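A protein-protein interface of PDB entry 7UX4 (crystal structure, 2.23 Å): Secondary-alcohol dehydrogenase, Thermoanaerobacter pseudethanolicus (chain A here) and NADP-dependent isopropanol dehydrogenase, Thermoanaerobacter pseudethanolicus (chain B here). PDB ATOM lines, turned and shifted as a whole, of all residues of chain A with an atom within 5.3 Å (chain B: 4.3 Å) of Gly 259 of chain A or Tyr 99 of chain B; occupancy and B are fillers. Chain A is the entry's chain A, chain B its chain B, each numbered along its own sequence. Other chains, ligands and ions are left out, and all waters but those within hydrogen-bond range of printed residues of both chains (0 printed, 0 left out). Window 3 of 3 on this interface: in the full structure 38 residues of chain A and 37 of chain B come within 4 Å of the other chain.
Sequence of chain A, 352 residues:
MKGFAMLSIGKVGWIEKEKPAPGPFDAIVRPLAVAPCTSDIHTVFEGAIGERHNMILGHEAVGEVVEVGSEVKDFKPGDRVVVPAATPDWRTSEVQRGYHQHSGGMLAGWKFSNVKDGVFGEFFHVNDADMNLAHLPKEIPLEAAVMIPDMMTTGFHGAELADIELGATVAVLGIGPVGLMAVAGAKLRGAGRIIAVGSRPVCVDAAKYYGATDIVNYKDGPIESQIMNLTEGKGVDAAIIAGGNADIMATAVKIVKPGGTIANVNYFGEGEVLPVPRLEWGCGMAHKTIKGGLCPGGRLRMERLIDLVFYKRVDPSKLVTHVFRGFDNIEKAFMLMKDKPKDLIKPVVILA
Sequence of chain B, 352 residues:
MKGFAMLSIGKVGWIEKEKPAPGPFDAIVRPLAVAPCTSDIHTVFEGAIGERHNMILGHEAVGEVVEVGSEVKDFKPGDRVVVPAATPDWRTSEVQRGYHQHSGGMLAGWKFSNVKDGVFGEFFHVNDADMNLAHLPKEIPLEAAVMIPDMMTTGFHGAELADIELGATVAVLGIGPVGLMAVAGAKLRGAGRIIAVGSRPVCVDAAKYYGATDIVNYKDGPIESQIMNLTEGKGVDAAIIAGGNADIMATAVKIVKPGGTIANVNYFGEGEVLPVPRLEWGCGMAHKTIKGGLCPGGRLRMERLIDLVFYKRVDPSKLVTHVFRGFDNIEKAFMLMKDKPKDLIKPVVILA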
ATOM      1  N   LYS A 257     -26.516   1.333 -12.627  1.00  0.00           N
ATOM      2  CA  LYS A 257     -26.909   1.763 -13.956  1.00  0.00           C
ATOM      3  C   LYS A 257     -27.829   0.731 -14.598  1.00  0.00           C
ATOM      4  O   LYS A 257     -27.864  -0.427 -14.175  1.00  0.00           O
ATOM      5  CB  LYS A 257     -25.672   1.973 -14.822  1.00  0.00           C
ATOM      6  CG  LYS A 257     -24.912   0.702 -15.127  1.00  0.00           C
ATOM      7  CD  LYS A 257     -23.682   1.000 -15.970  1.00  0.00           C
ATOM      8  CE  LYS A 257     -22.696   1.869 -15.217  1.00  0.00           C
ATOM      9  NZ  LYS A 257     -21.409   1.990 -15.959  1.00  0.00           N
ATOM     10  N   PRO A 258     -28.597   1.128 -15.615  1.00  0.00           N
ATOM     11  CA  PRO A 258     -29.456   0.159 -16.307  1.00  0.00           C
ATOM     12  C   PRO A 258     -28.631  -0.986 -16.872  1.00  0.00           C
ATOM     13  O   PRO A 258     -27.594  -0.773 -17.505  1.00  0.00           O
ATOM     14  CB  PRO A 258     -30.109   0.991 -17.414  1.00  0.00           C
ATOM     15  CG  PRO A 258     -30.081   2.382 -16.902  1.00  0.00           C
ATOM     16  CD  PRO A 258     -28.806   2.498 -16.114  1.00  0.00           C
ATOM     17  N   GLY A 259     -29.096  -2.209 -16.636  1.00  0.00           N
ATOM     18  CA  GLY A 259     -28.346  -3.387 -17.007  1.00  0.00           C
ATOM     19  C   GLY A 259     -27.415  -3.909 -15.935  1.00  0.00           C
ATOM     20  O   GLY A 259     -26.848  -4.995 -16.107  1.00  0.00           O
ATOM     21  N   GLY A 260     -27.243  -3.179 -14.836  1.00  0.00           N
ATOM     22  CA  GLY A 260     -26.384  -3.608 -13.754  1.00  0.00           C
ATOM     23  C   GLY A 260     -27.066  -4.613 -12.844  1.00  0.00           C
ATOM     24  O   GLY A 260     -28.117  -5.173 -13.154  1.00  0.00           O
ATOM     25  N   THR A 261     -26.446  -4.835 -11.684  1.00  0.00           N
ATOM     26  CA  THR A 261     -26.887  -5.870 -10.757  1.00  0.00           C
ATOM     27  C   THR A 261     -26.811  -5.366  -9.321  1.00  0.00           C
ATOM     28  O   THR A 261     -25.843  -4.703  -8.937  1.00  0.00           O
ATOM     29  CB  THR A 261     -26.032  -7.140 -10.903  1.00  0.00           C
ATOM     30  OG1 THR A 261     -26.073  -7.596 -12.262  1.00  0.00           O
ATOM     31  CG2 THR A 261     -26.546  -8.248  -9.988  1.00  0.00           C
ATOM     32  N   ALA A 286     -35.828  -1.834 -16.322  1.00  0.00           N
ATOM     33  CA  ALA A 286     -34.505  -1.233 -16.451  1.00  0.00           C
ATOM     34  C   ALA A 286     -33.375  -2.255 -16.508  1.00  0.00           C
ATOM     35  O   ALA A 286     -32.207  -1.854 -16.565  1.00  0.00           O
ATOM     36  CB  ALA A 286     -34.252  -0.264 -15.294  1.00  0.00           C
ATOM     37  N   HIS A 287     -33.690  -3.553 -16.508  1.00  0.00           N
ATOM     38  CA  HIS A 287     -32.687  -4.625 -16.511  1.00  0.00           C
ATOM     39  C   HIS A 287     -31.711  -4.507 -15.340  1.00  0.00           C
ATOM     40  O   HIS A 287     -30.526  -4.820 -15.467  1.00  0.00           O
ATOM     41  CB  HIS A 287     -31.924  -4.679 -17.838  1.00  0.00           C
ATOM     42  CG  HIS A 287     -32.730  -5.229 -18.973  1.00  0.00           C
ATOM     43  ND1 HIS A 287     -33.374  -4.424 -19.888  1.00  0.00           N
ATOM     44  CD2 HIS A 287     -33.016  -6.504 -19.328  1.00  0.00           C
ATOM     45  CE1 HIS A 287     -34.007  -5.179 -20.769  1.00  0.00           C
ATOM     46  NE2 HIS A 287     -33.811  -6.445 -20.448  1.00  0.00           N
ATOM     47  N   LYS A 288     -32.204  -4.053 -14.191  1.00  0.00           N
ATOM     48  CA  LYS A 288     -31.411  -4.012 -12.961  1.00  0.00           C
ATOM     49  C   LYS A 288     -31.727  -5.282 -12.178  1.00  0.00           C
ATOM     50  O   LYS A 288     -32.734  -5.353 -11.469  1.00  0.00           O
ATOM     51  CB  LYS A 288     -31.706  -2.756 -12.145  1.00  0.00           C
ATOM     52  CG  LYS A 288     -31.396  -1.437 -12.858  1.00  0.00           C
ATOM     53  CD  LYS A 288     -31.494  -0.258 -11.893  1.00  0.00           C
ATOM     54  CE  LYS A 288     -31.321   1.062 -12.615  1.00  0.00           C
ATOM     55  NZ  LYS A 288     -31.248   2.204 -11.664  1.00  0.00           N
ATOM     56  N   GLU B  94     -24.010   1.866 -24.001  1.00  0.00           N
ATOM     57  CA  GLU B  94     -24.888   0.818 -23.483  1.00  0.00           C
ATOM     58  C   GLU B  94     -24.999  -0.353 -24.449  1.00  0.00           C
ATOM     59  O   GLU B  94     -25.249  -1.486 -24.019  1.00  0.00           O
ATOM     60  CB  GLU B  94     -26.280   1.374 -23.174  1.00  0.00           C
ATOM     61  CG  GLU B  94     -26.336   2.283 -21.954  1.00  0.00           C
ATOM     62  CD  GLU B  94     -26.080   3.743 -22.290  1.00  0.00           C
ATOM     63  OE1 GLU B  94     -26.087   4.094 -23.491  1.00  0.00           O
ATOM     64  OE2 GLU B  94     -25.869   4.538 -21.348  1.00  0.00           O
ATOM     65  N   ARG B  97     -22.163  -2.538 -23.791  1.00  0.00           N
ATOM     66  CA  ARG B  97     -22.421  -3.318 -22.585  1.00  0.00           C
ATOM     67  C   ARG B  97     -23.431  -4.437 -22.803  1.00  0.00           C
ATOM     68  O   ARG B  97     -23.608  -5.272 -21.906  1.00  0.00           O
ATOM     69  CB  ARG B  97     -22.916  -2.415 -21.442  1.00  0.00           C
ATOM     70  CG  ARG B  97     -21.822  -1.628 -20.746  1.00  0.00           C
ATOM     71  CD  ARG B  97     -22.236  -1.155 -19.357  1.00  0.00           C
ATOM     72  NE  ARG B  97     -23.327  -0.186 -19.375  1.00  0.00           N
ATOM     73  CZ  ARG B  97     -24.572  -0.439 -18.989  1.00  0.00           C
ATOM     74  NH1 ARG B  97     -24.931  -1.634 -18.547  1.00  0.00           N
ATOM     75  NH2 ARG B  97     -25.473   0.538 -19.029  1.00  0.00           N
ATOM     76  N   GLY B  98     -24.104  -4.466 -23.951  1.00  0.00           N
ATOM     77  CA  GLY B  98     -25.053  -5.520 -24.250  1.00  0.00           C
ATOM     78  C   GLY B  98     -26.489  -5.218 -23.900  1.00  0.00           C
ATOM     79  O   GLY B  98     -27.292  -6.151 -23.783  1.00  0.00           O
ATOM     80  N   TYR B  99     -26.845  -3.941 -23.728  1.00  0.00           N
ATOM     81  CA  TYR B  99     -28.198  -3.528 -23.342  1.00  0.00           C
ATOM     82  C   TYR B  99     -28.647  -2.411 -24.281  1.00  0.00           C
ATOM     83  O   TYR B  99     -28.670  -1.236 -23.908  1.00  0.00           O
ATOM     84  CB  TYR B  99     -28.243  -3.098 -21.874  1.00  0.00           C
ATOM     85  CG  TYR B  99     -28.065  -4.244 -20.908  1.00  0.00           C
ATOM     86  CD1 TYR B  99     -29.150  -5.028 -20.530  1.00  0.00           C
ATOM     87  CD2 TYR B  99     -26.816  -4.552 -20.379  1.00  0.00           C
ATOM     88  CE1 TYR B  99     -28.997  -6.086 -19.647  1.00  0.00           C
ATOM     89  CE2 TYR B  99     -26.653  -5.611 -19.495  1.00  0.00           C
ATOM     90  CZ  TYR B  99     -27.749  -6.374 -19.133  1.00  0.00           C
ATOM     91  OH  TYR B  99     -27.604  -7.429 -18.256  1.00  0.00           O
ATOM     92  N   HIS B 100     -29.009  -2.787 -25.510  1.00  0.00           N
ATOM     93  CA  HIS B 100     -29.471  -1.800 -26.476  1.00  0.00           C
ATOM     94  C   HIS B 100     -30.799  -1.176 -26.067  1.00  0.00           C
ATOM     95  O   HIS B 100     -31.090  -0.046 -26.479  1.00  0.00           O
ATOM     96  CB  HIS B 100     -29.585  -2.433 -27.866  1.00  0.00           C
ATOM     97  CG  HIS B 100     -30.675  -3.455 -27.983  1.00  0.00           C
ATOM     98  ND1 HIS B 100     -30.450  -4.806 -27.832  1.00  0.00           N
ATOM     99  CD2 HIS B 100     -32.000  -3.321 -28.232  1.00  0.00           C
ATOM    100  CE1 HIS B 100     -31.587  -5.460 -27.986  1.00  0.00           C
ATOM    101  NE2 HIS B 100     -32.543  -4.583 -28.229  1.00  0.00           N
ATOM    102  N   GLN B 101     -31.597  -1.868 -25.244  1.00  0.00           N
ATOM    103  CA  GLN B 101     -32.859  -1.302 -24.777  1.00  0.00           C
ATOM    104  C   GLN B 101     -32.661   0.014 -24.046  1.00  0.00           C
ATOM    105  O   GLN B 101     -33.607   0.803 -23.947  1.00  0.00           O
ATOM    106  CB  GLN B 101     -33.586  -2.274 -23.846  1.00  0.00           C
ATOM    107  CG  GLN B 101     -33.962  -3.615 -24.463  1.00  0.00           C
ATOM    108  CD  GLN B 101     -32.934  -4.692 -24.182  1.00  0.00           C
ATOM    109  OE1 GLN B 101     -31.729  -4.443 -24.236  1.00  0.00           O
ATOM    110  NE2 GLN B 101     -33.403  -5.893 -23.865  1.00  0.00           N
ATOM    111  N   HIS B 102     -31.463   0.261 -23.518  1.00  0.00           N
ATOM    112  CA  HIS B 102     -31.163   1.467 -22.757  1.00  0.00           C
ATOM    113  C   HIS B 102     -30.094   2.310 -23.443  1.00  0.00           C
ATOM    114  O   HIS B 102     -29.324   3.015 -22.786  1.00  0.00           O
ATOM    115  CB  HIS B 102     -30.754   1.087 -21.337  1.00  0.00           C
ATOM    116  CG  HIS B 102     -31.671   0.081 -20.716  1.00  0.00           C
ATOM    117  ND1 HIS B 102     -32.961   0.386 -20.338  1.00  0.00           N
ATOM    118  CD2 HIS B 102     -31.508  -1.240 -20.466  1.00  0.00           C
ATOM    119  CE1 HIS B 102     -33.543  -0.696 -19.851  1.00  0.00           C
ATOM    120  NE2 HIS B 102     -32.682  -1.696 -19.919  1.00  0.00           N
ATOM    121  N   SER B 103     -30.048   2.248 -24.770  1.00  0.00           N
ATOM    122  CA  SER B 103     -29.065   2.985 -25.553  1.00  0.00           C
ATOM    123  C   SER B 103     -29.353   4.478 -25.452  1.00  0.00           C
ATOM    124  O   SER B 103     -30.324   4.969 -26.038  1.00  0.00           O
ATOM    125  CB  SER B 103     -29.100   2.507 -27.000  1.00  0.00           C
ATOM    126  OG  SER B 103     -28.279   3.306 -27.826  1.00  0.00           O
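Printed residues of chain A that touch a printed residue of chain B: Lys 257, Pro 258, Gly 259, Ala 286 and His 287.
Hydrophobic or aromatic side chains of chain A that line the printed part of chain B: Pro 258 and His 287.
Of the 8 printed residues of chain B, 4 touch a printed residue of chain A.
Hydrophobic or aromatic side chains of chain B within 4 Å of the printed part of chain A: Tyr 99 and His 102.
Along chain B the printed residues that touch a printed residue of chain A span positions 97 to 102.
Of the printed residues of chain B, Lys 257 of chain A touches Arg 97.
Of the printed residues of chain B, Pro 258 of chain A touches Arg 97 (2.9 Å) and His 102 (3.8 Å).
Of chain B, only Tyr 99 comes within 4 Å of Gly 259 of chain A.
Of the printed residues of chain B, Ala 286 of chain A touches His 102.
Of the printed residues of chain A, Arg 97 of chain B touches Lys 257 and Pro 258.
Of chain A, only Gly 259 and His 287 come within 4 Å of Tyr 99 of chain B.
His 100 of chain B touches none of the printed residues of chain A.
Of the printed residues of chain A, Gln 101 of chain B touches His 287 (3.2 Å).
Ser 103 of chain B touches none of the printed residues of chain A.
The nearest residue of chain A that does not touch Tyr 99 of chain B is Pro 258 of chain A (4.8 Å).
NH2 of Arg 97 of chain B lies within hydrogen-bond range of O of Pro 258 of chain A (2.9 Å).
The backbone carbonyl oxygen (O) of Gly 259 of chain A is in hydrogen-bond range of the side-chain hydroxyl (OH) of Tyr 99 of chain B (3.3 Å).
NE2 of His 102 of chain B lies within hydrogen-bond range of O of Ala 286 of chain A (3.4 Å).
A ring nitrogen (NE2) of His 287 of chain A sits close to the side-chain amide nitrogen of Gln 101 of chain B, at 3.5 Å.
A ring nitrogen (NE2) of His 102 of chain B is in hydrogen-bond range of a ring nitrogen (ND1) of His 287 of chain A.
CD of Lys 257 of chain A touches CZ of Arg 97 of chain B (3.5 Å).
His 102 of chain B touches Pro 258 of chain A.
His 287 of chain A touches Tyr 99 of chain B.
The backbone NH (N) of Gly 259 of chain A is in hydrogen-bond range of the backbone carbonyl oxygen (O) of Ala 286 of chain A (3.1 Å).
The backbone NH (N) of Gly 259 of chain A lies close to the backbone carbonyl oxygen (O) of His 287 of chain A, 3.2 Å away.
O of Glu 94 of chain B is in hydrogen-bond range of N of Tyr 99 of chain B.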
